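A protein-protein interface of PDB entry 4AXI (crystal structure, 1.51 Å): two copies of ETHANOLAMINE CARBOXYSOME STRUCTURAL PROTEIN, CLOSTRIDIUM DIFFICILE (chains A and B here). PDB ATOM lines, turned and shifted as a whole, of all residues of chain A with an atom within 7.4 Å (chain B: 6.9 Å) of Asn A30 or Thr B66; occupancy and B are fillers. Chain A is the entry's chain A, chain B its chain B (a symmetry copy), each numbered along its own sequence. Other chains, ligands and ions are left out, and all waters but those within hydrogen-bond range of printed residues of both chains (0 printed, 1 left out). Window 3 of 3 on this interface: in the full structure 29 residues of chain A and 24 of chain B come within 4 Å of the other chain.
The backbone NH (N) of Ile A26 lies within hydrogen-bond range of the backbone carbonyl oxygen (O) of Ile A47, 2.9 Å away. OD1 of Asn A30 lies within hydrogen-bond range of N of Asp A32 (2.7 Å). The side-chain amide oxygen (OD1) of Asn A30 sits close to the backbone NH (N) of Ile A33. The side-chain hydroxyl (OG1) of Thr B66 lies within hydrogen-bond range of the backbone carbonyl oxygen (O) of Ala B62 (3.1 Å). The side-chain hydroxyl (OG1) of Thr B66 sits at hydrogen-bond distance from the backbone carbonyl oxygen (O) of Asp B63, at 3.2 Å. The side-chain amino group of Lys B67 is in salt-bridge range of the side-chain carboxylate of Asp B63 (2.9 Å).
NZ of Lys B67 is in hydrogen-bond range of O of Asn A28 (2.9 Å). N of Asn A30 sits at hydrogen-bond distance from OD1 of Asp B63. The side-chain amide nitrogen of Asn A30 lies within hydrogen-bond range of the side-chain hydroxyl of Thr B66 (3.2 Å).
Among the printed residues, pairs that only touch across the chains: Ile A26 with Asp B63, Ile A26 with Lys B67, Pro A29 with Asp B63, Ile A33 with Ala B62, Ile A33 with Asp B63 and Ile A33 with Thr B66.
No position is printed for both chains.
Printed residues of chain B that touch a printed residue of chain A: Ala B62, Asp B63, Thr B66 and Lys B67. Hydrophobic or aromatic side chains of chain B within 4 Å of the printed part of chain A: Ala B62. Printed residues of chain A that touch a printed residue of chain B: Ile A26, Asn A28, Pro A29, Asn A30 and Ile A33. Hydrophobic or aromatic side chains of chain A within 4 Å of the printed part of chain B: Ile A26 and Ile A33. Along chain A the printed residues that touch a printed residue of chain B span positions 26 to 33. Among the printed residues, 9 pairs touch across the chains. Among the printed residues, no Asp or Glu carboxylate lies within 4 Å of a Lys or Arg side-chain nitrogen of the other chain.
Printed residues of chain B within 4 Å of Pro A29: Asp B63. Asn A30 touches just these residues of chain B: Asp B63 and Thr B66. Of the printed residues of chain B, Ile A33 touches Ala B62, Asp B63 and Thr B66. Tyr A34 touches none of the printed residues of chain B. No residue of chain A comes within 4 Å of Ala B65. Of chain A, only Asn A30 and Ile A33 come within 4 Å of Thr B66. Ala B68 touches none of the printed residues of chain A. The nearest printed residue of chain B that does not touch Ile A26 is Ala B61 (6.2 Å).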
ATOM      1  N   ILE A  26       9.424  13.626  15.069  1.00  0.00           N
ATOM      2  CA  ILE A  26       8.662  14.841  15.349  1.00  0.00           C
ATOM      3  C   ILE A  26       8.614  15.641  14.055  1.00  0.00           C
ATOM      4  O   ILE A  26       9.632  16.211  13.621  1.00  0.00           O
ATOM      5  CB  ILE A  26       9.286  15.702  16.467  1.00  0.00           C
ATOM      6  CG1 ILE A  26       9.407  14.893  17.756  1.00  0.00           C
ATOM      7  CG2 ILE A  26       8.408  16.906  16.745  1.00  0.00           C
ATOM      8  CD1 ILE A  26       9.961  15.642  18.940  1.00  0.00           C
ATOM      9  N   ALA A  27       7.423  15.772  13.475  1.00  0.00           N
ATOM     10  CA  ALA A  27       7.309  16.411  12.150  1.00  0.00           C
ATOM     11  C   ALA A  27       7.570  17.892  12.059  1.00  0.00           C
ATOM     12  O   ALA A  27       8.072  18.381  11.003  1.00  0.00           O
ATOM     13  CB  ALA A  27       5.935  16.117  11.494  1.00  0.00           C
ATOM     14  N   ASN A  28       7.180  18.632  13.080  1.00  0.00           N
ATOM     15  CA  ASN A  28       7.322  20.072  12.973  1.00  0.00           C
ATOM     16  C   ASN A  28       7.715  20.578  14.310  1.00  0.00           C
ATOM     17  O   ASN A  28       6.912  21.133  15.053  1.00  0.00           O
ATOM     18  CB  ASN A  28       6.024  20.737  12.531  1.00  0.00           C
ATOM     19  CG  ASN A  28       6.160  22.252  12.460  1.00  0.00           C
ATOM     20  OD1 ASN A  28       7.278  22.785  12.534  1.00  0.00           O
ATOM     21  ND2 ASN A  28       5.045  22.951  12.321  1.00  0.00           N
ATOM     22  N   PRO A  29       8.980  20.352  14.638  1.00  0.00           N
ATOM     23  CA  PRO A  29       9.368  20.585  16.020  1.00  0.00           C
ATOM     24  C   PRO A  29       9.368  22.044  16.389  1.00  0.00           C
ATOM     25  O   PRO A  29       9.676  22.914  15.562  1.00  0.00           O
ATOM     26  CB  PRO A  29      10.777  19.987  16.097  1.00  0.00           C
ATOM     27  CG  PRO A  29      11.272  20.014  14.713  1.00  0.00           C
ATOM     28  CD  PRO A  29      10.074  19.796  13.823  1.00  0.00           C
ATOM     29  N   ASN A  30       8.938  22.320  17.613  1.00  0.00           N
ATOM     30  CA  ASN A  30       8.944  23.685  18.136  1.00  0.00           C
ATOM     31  C   ASN A  30      10.347  24.281  18.154  1.00  0.00           C
ATOM     32  O   ASN A  30      11.280  23.638  18.621  1.00  0.00           O
ATOM     33  CB  ASN A  30       8.351  23.602  19.538  1.00  0.00           C
ATOM     34  CG  ASN A  30       8.498  24.874  20.340  1.00  0.00           C
ATOM     35  OD1 ASN A  30       9.586  25.216  20.829  1.00  0.00           O
ATOM     36  ND2 ASN A  30       7.392  25.507  20.583  1.00  0.00           N
ATOM     37  N   GLU A  31      10.499  25.503  17.648  1.00  0.00           N
ATOM     38  CA  GLU A  31      11.811  26.131  17.558  1.00  0.00           C
ATOM     39  C   GLU A  31      12.518  26.282  18.899  1.00  0.00           C
ATOM     40  O   GLU A  31      13.742  26.207  18.939  1.00  0.00           O
ATOM     41  CB  GLU A  31      11.765  27.498  16.858  1.00  0.00           C
ATOM     42  CG  GLU A  31      11.296  28.650  17.743  1.00  0.00           C
ATOM     43  CD  GLU A  31      11.387  30.027  17.055  1.00  0.00           C
ATOM     44  OE1 GLU A  31      12.459  30.366  16.487  1.00  0.00           O
ATOM     45  OE2 GLU A  31      10.378  30.768  17.093  1.00  0.00           O
ATOM     46  N   ASP A  32      11.798  26.524  19.992  1.00  0.00           N
ATOM     47  CA  ASP A  32      12.497  26.675  21.279  1.00  0.00           C
ATOM     48  C   ASP A  32      13.127  25.351  21.679  1.00  0.00           C
ATOM     49  O   ASP A  32      14.206  25.324  22.276  1.00  0.00           O
ATOM     50  CB  ASP A  32      11.565  27.181  22.375  1.00  0.00           C
ATOM     51  CG  ASP A  32      10.913  28.505  22.012  1.00  0.00           C
ATOM     52  OD1 ASP A  32      11.656  29.512  21.965  1.00  0.00           O
ATOM     53  OD2 ASP A  32       9.677  28.547  21.780  1.00  0.00           O
ATOM     54  N   ILE A  33      12.479  24.247  21.324  1.00  0.00           N
ATOM     55  CA  ILE A  33      13.004  22.950  21.664  1.00  0.00           C
ATOM     56  C   ILE A  33      14.217  22.705  20.791  1.00  0.00           C
ATOM     57  O   ILE A  33      15.268  22.319  21.282  1.00  0.00           O
ATOM     58  CB  ILE A  33      11.962  21.832  21.447  1.00  0.00           C
ATOM     59  CG1 ILE A  33      10.946  21.784  22.584  1.00  0.00           C
ATOM     60  CG2 ILE A  33      12.654  20.467  21.439  1.00  0.00           C
ATOM     61  CD1 ILE A  33      10.166  22.961  22.758  1.00  0.00           C
ATOM     62  N   TYR A  34      14.115  22.890  19.485  1.00  0.00           N
ATOM     63  CA  TYR A  34      15.239  22.442  18.684  1.00  0.00           C
ATOM     64  C   TYR A  34      16.449  23.354  18.829  1.00  0.00           C
ATOM     65  O   TYR A  34      17.585  22.907  18.687  1.00  0.00           O
ATOM     66  CB  TYR A  34      14.881  22.115  17.226  1.00  0.00           C
ATOM     67  CG  TYR A  34      14.501  23.243  16.280  1.00  0.00           C
ATOM     68  CD1 TYR A  34      15.431  24.181  15.869  1.00  0.00           C
ATOM     69  CD2 TYR A  34      13.224  23.310  15.727  1.00  0.00           C
ATOM     70  CE1 TYR A  34      15.096  25.184  14.972  1.00  0.00           C
ATOM     71  CE2 TYR A  34      12.880  24.313  14.838  1.00  0.00           C
ATOM     72  CZ  TYR A  34      13.828  25.238  14.454  1.00  0.00           C
ATOM     73  OH  TYR A  34      13.490  26.252  13.571  1.00  0.00           O
ATOM     74  N   LYS A  35      16.210  24.610  19.178  1.00  0.00           N
ATOM     75  CA  LYS A  35      17.334  25.494  19.450  1.00  0.00           C
ATOM     76  C   LYS A  35      18.052  25.128  20.757  1.00  0.00           C
ATOM     77  O   LYS A  35      19.260  25.229  20.855  1.00  0.00           O
ATOM     78  CB  LYS A  35      16.896  26.971  19.397  1.00  0.00           C
ATOM     79  CG  LYS A  35      16.783  27.472  17.933  1.00  0.00           C
ATOM     80  CD  LYS A  35      16.255  28.911  17.791  1.00  0.00           C
ATOM     81  CE  LYS A  35      16.244  29.332  16.311  1.00  0.00           C
ATOM     82  NZ  LYS A  35      15.866  30.770  16.060  1.00  0.00           N
ATOM     83  N   LYS A  36      17.323  24.683  21.769  1.00  0.00           N
ATOM     84  CA  LYS A  36      17.958  24.228  22.981  1.00  0.00           C
ATOM     85  C   LYS A  36      18.794  22.963  22.738  1.00  0.00           C
ATOM     86  O   LYS A  36      19.738  22.712  23.469  1.00  0.00           O
ATOM     87  CB  LYS A  36      16.865  24.033  24.054  1.00  0.00           C
ATOM     88  CG  LYS A  36      17.351  23.450  25.349  1.00  0.00           C
ATOM     89  CD  LYS A  36      18.572  24.179  25.863  1.00  0.00           C
ATOM     90  CE  LYS A  36      19.326  23.350  26.893  1.00  0.00           C
ATOM     91  NZ  LYS A  36      19.541  21.969  26.430  1.00  0.00           N
ATOM     92  N   LEU A  41      17.605  24.187  11.570  1.00  0.00           N
ATOM     93  CA  LEU A  41      16.718  23.438  10.694  1.00  0.00           C
ATOM     94  C   LEU A  41      16.022  24.363   9.724  1.00  0.00           C
ATOM     95  O   LEU A  41      15.968  25.561   9.945  1.00  0.00           O
ATOM     96  CB  LEU A  41      15.628  22.804  11.527  1.00  0.00           C
ATOM     97  CG  LEU A  41      16.035  21.824  12.616  1.00  0.00           C
ATOM     98  CD1 LEU A  41      14.761  21.369  13.326  1.00  0.00           C
ATOM     99  CD2 LEU A  41      16.757  20.642  12.006  1.00  0.00           C
ATOM    100  N   ILE A  47      12.459  16.091  12.818  1.00  0.00           N
ATOM    101  CA  ILE A  47      13.592  15.430  13.446  1.00  0.00           C
ATOM    102  C   ILE A  47      13.269  13.996  13.789  1.00  0.00           C
ATOM    103  O   ILE A  47      12.105  13.630  13.984  1.00  0.00           O
ATOM    104  CB  ILE A  47      14.112  16.166  14.682  1.00  0.00           C
ATOM    105  CG1 ILE A  47      13.077  16.297  15.752  1.00  0.00           C
ATOM    106  CG2 ILE A  47      14.615  17.574  14.330  1.00  0.00           C
ATOM    107  CD1 ILE A  47      13.691  16.894  17.106  1.00  0.00           C
ATOM    108  N   ALA B  61       8.427  15.054  24.965  1.00  0.00           N
ATOM    109  CA  ALA B  61       7.560  15.686  25.927  1.00  0.00           C
ATOM    110  C   ALA B  61       7.579  17.195  25.823  1.00  0.00           C
ATOM    111  O   ALA B  61       6.543  17.835  25.956  1.00  0.00           O
ATOM    112  CB  ALA B  61       7.977  15.254  27.334  1.00  0.00           C
ATOM    113  N   ALA B  62       8.773  17.788  25.724  1.00  0.00           N
ATOM    114  CA  ALA B  62       8.884  19.252  25.669  1.00  0.00           C
ATOM    115  C   ALA B  62       8.168  19.813  24.451  1.00  0.00           C
ATOM    116  O   ALA B  62       7.516  20.857  24.523  1.00  0.00           O
ATOM    117  CB  ALA B  62      10.322  19.642  25.650  1.00  0.00           C
ATOM    118  N   ASP B  63       8.298  19.129  23.330  1.00  0.00           N
ATOM    119  CA  ASP B  63       7.634  19.554  22.114  1.00  0.00           C
ATOM    120  C   ASP B  63       6.124  19.454  22.274  1.00  0.00           C
ATOM    121  O   ASP B  63       5.387  20.399  21.930  1.00  0.00           O
ATOM    122  CB  ASP B  63       8.111  18.674  20.975  1.00  0.00           C
ATOM    123  CG  ASP B  63       7.494  19.045  19.690  1.00  0.00           C
ATOM    124  OD1 ASP B  63       7.881  20.106  19.180  1.00  0.00           O
ATOM    125  OD2 ASP B  63       6.636  18.279  19.209  1.00  0.00           O
ATOM    126  N   VAL B  64       5.627  18.333  22.785  1.00  0.00           N
ATOM    127  CA  VAL B  64       4.191  18.181  22.996  1.00  0.00           C
ATOM    128  C   VAL B  64       3.662  19.255  23.949  1.00  0.00           C
ATOM    129  O   VAL B  64       2.575  19.866  23.683  1.00  0.00           O
ATOM    130  CB  VAL B  64       3.880  16.762  23.516  1.00  0.00           C
ATOM    131  CG1 VAL B  64       2.464  16.660  24.110  1.00  0.00           C
ATOM    132  CG2 VAL B  64       4.101  15.700  22.388  1.00  0.00           C
ATOM    133  N   ALA B  65       4.402  19.523  25.030  1.00  0.00           N
ATOM    134  CA  ALA B  65       3.916  20.440  26.049  1.00  0.00           C
ATOM    135  C   ALA B  65       3.788  21.830  25.461  1.00  0.00           C
ATOM    136  O   ALA B  65       2.734  22.463  25.602  1.00  0.00           O
ATOM    137  CB  ALA B  65       4.870  20.465  27.215  1.00  0.00           C
ATOM    138  N   THR B  66       4.823  22.282  24.739  1.00  0.00           N
ATOM    139  CA  THR B  66       4.800  23.622  24.153  1.00  0.00           C
ATOM    140  C   THR B  66       3.791  23.778  23.028  1.00  0.00           C
ATOM    141  O   THR B  66       3.319  24.912  22.801  1.00  0.00           O
ATOM    142  CB  THR B  66       6.191  24.085  23.687  1.00  0.00           C
ATOM    143  OG1 THR B  66       6.704  23.185  22.696  1.00  0.00           O
ATOM    144  CG2 THR B  66       7.141  24.184  24.857  1.00  0.00           C
ATOM    145  N   LYS B  67       3.425  22.699  22.343  1.00  0.00           N
ATOM    146  CA  LYS B  67       2.352  22.767  21.330  1.00  0.00           C
ATOM    147  C   LYS B  67       0.964  22.693  21.977  1.00  0.00           C
ATOM    148  O   LYS B  67      -0.020  23.146  21.432  1.00  0.00           O
ATOM    149  CB  LYS B  67       2.503  21.613  20.351  1.00  0.00           C
ATOM    150  CG  LYS B  67       3.677  21.738  19.482  1.00  0.00           C
ATOM    151  CD  LYS B  67       3.864  20.515  18.627  1.00  0.00           C
ATOM    152  CE  LYS B  67       4.991  20.774  17.619  1.00  0.00           C
ATOM    153  NZ  LYS B  67       5.449  19.522  16.921  1.00  0.00           N
ATOM    154  N   ALA B  68       0.895  22.074  23.146  1.00  0.00           N
ATOM    155  CA  ALA B  68      -0.363  21.767  23.794  1.00  0.00           C
ATOM    156  C   ALA B  68      -1.053  23.065  24.201  1.00  0.00           C
ATOM    157  O   ALA B  68      -2.272  23.249  23.997  1.00  0.00           O
ATOM    158  CB  ALA B  68      -0.074  20.846  25.032  1.00  0.00           C
ATOM    159  N   SER B  69      -0.273  23.976  24.755  1.00  0.00           N
ATOM    160  CA  SER B  69      -0.841  25.130  25.429  1.00  0.00           C
ATOM    161  C   SER B  69       0.166  26.216  25.610  1.00  0.00           C
ATOM    162  O   SER B  69       1.268  26.152  25.140  1.00  0.00           O
ATOM    163  CB  SER B  69      -1.373  24.742  26.794  1.00  0.00           C
ATOM    164  OG  SER B  69      -0.295  24.243  27.537  1.00  0.00           O
ATOM    165  N   ASN B  70      -0.250  27.252  26.309  1.00  0.00           N
ATOM    166  CA  ASN B  70       0.566  28.431  26.444  1.00  0.00           C
ATOM    167  C   ASN B  70       1.525  28.330  27.613  1.00  0.00           C
ATOM    168  O   ASN B  70       1.413  29.041  28.616  1.00  0.00           O
ATOM    169  CB  ASN B  70      -0.358  29.624  26.659  1.00  0.00           C
ATOM    170  CG  ASN B  70       0.387  30.948  26.646  1.00  0.00           C
ATOM    171  OD1 ASN B  70       1.392  31.111  25.960  1.00  0.00           O
ATOM    172  ND2 ASN B  70      -0.131  31.928  27.421  1.00  0.00           N
ATOM    173  N   VAL B  71       2.483  27.417  27.467  1.00  0.00           N
ATOM    174  CA  VAL B  71       3.536  27.216  28.450  1.00  0.00           C
ATOM    175  C   VAL B  71       4.856  27.540  27.803  1.00  0.00           C
ATOM    176  O   VAL B  71       5.023  27.456  26.551  1.00  0.00           O
ATOM    177  CB  VAL B  71       3.561  25.765  29.036  1.00  0.00           C
ATOM    178  CG1 VAL B  71       2.240  25.472  29.736  1.00  0.00           C
ATOM    179  CG2 VAL B  71       3.869  24.757  27.965  1.00  0.00           C
ATOM    180  N   SER B  72       5.778  27.962  28.655  1.00  0.00           N
ATOM    181  CA  SER B  72       7.140  28.224  28.257  1.00  0.00           C
ATOM    182  C   SER B  72       7.969  27.043  28.745  1.00  0.00           C
ATOM    183  O   SER B  72       7.732  26.451  29.816  1.00  0.00           O
ATOM    184  CB  SER B  72       7.679  29.503  28.894  1.00  0.00           C
ATOM    185  OG  SER B  72       6.861  30.604  28.500  1.00  0.00           O
ATOM    186  N   LEU B  73       8.962  26.696  27.956  1.00  0.00           N
ATOM    187  CA  LEU B  73       9.929  25.710  28.379  1.00  0.00           C
ATOM    188  C   LEU B  73      10.949  26.302  29.319  1.00  0.00           C
ATOM    189  O   LEU B  73      11.726  27.181  28.919  1.00  0.00           O
ATOM    190  CB  LEU B  73      10.637  25.109  27.166  1.00  0.00           C
ATOM    191  CG  LEU B  73      11.664  24.015  27.491  1.00  0.00           C
ATOM    192  CD1 LEU B  73      11.030  22.796  28.136  1.00  0.00           C
ATOM    193  CD2 LEU B  73      12.385  23.601  26.191  1.00  0.00           C
ATOM    194  N   ILE B  85       8.362  23.078  32.827  1.00  0.00           N
ATOM    195  CA  ILE B  85       7.588  24.063  32.040  1.00  0.00           C
ATOM    196  C   ILE B  85       6.956  25.041  33.015  1.00  0.00           C
ATOM    197  O   ILE B  85       6.860  24.775  34.228  1.00  0.00           O
ATOM    198  CB  ILE B  85       6.525  23.388  31.176  1.00  0.00           C
ATOM    199  CG1 ILE B  85       5.506  22.611  32.031  1.00  0.00           C
ATOM    200  CG2 ILE B  85       7.196  22.540  30.143  1.00  0.00           C
ATOM    201  CD1 ILE B  85       4.320  21.994  31.267  1.00  0.00           C
ATOM    202  N   ALA B  95      -0.830  20.921  29.276  1.00  0.00           N
ATOM    203  CA  ALA B  95       0.448  20.432  28.735  1.00  0.00           C
ATOM    204  C   ALA B  95       0.818  19.070  29.340  1.00  0.00           C
ATOM    205  O   ALA B  95       1.187  18.143  28.600  1.00  0.00           O
ATOM    206  CB  ALA B  95       1.534  21.464  28.986  1.00  0.00           C
ATOM    207  N   VAL B  99       1.246  15.458  27.386  1.00  0.00           N
ATOM    208  CA  VAL B  99       2.480  14.671  27.462  1.00  0.00           C
ATOM    209  C   VAL B  99       2.164  13.245  27.890  1.00  0.00           C
ATOM    210  O   VAL B  99       2.659  12.259  27.324  1.00  0.00           O
ATOM    211  CB  VAL B  99       3.493  15.287  28.451  1.00  0.00           C
ATOM    212  CG1 VAL B  99       4.596  14.285  28.763  1.00  0.00           C
ATOM    213  CG2 VAL B  99       4.047  16.573  27.872  1.00  0.00           C
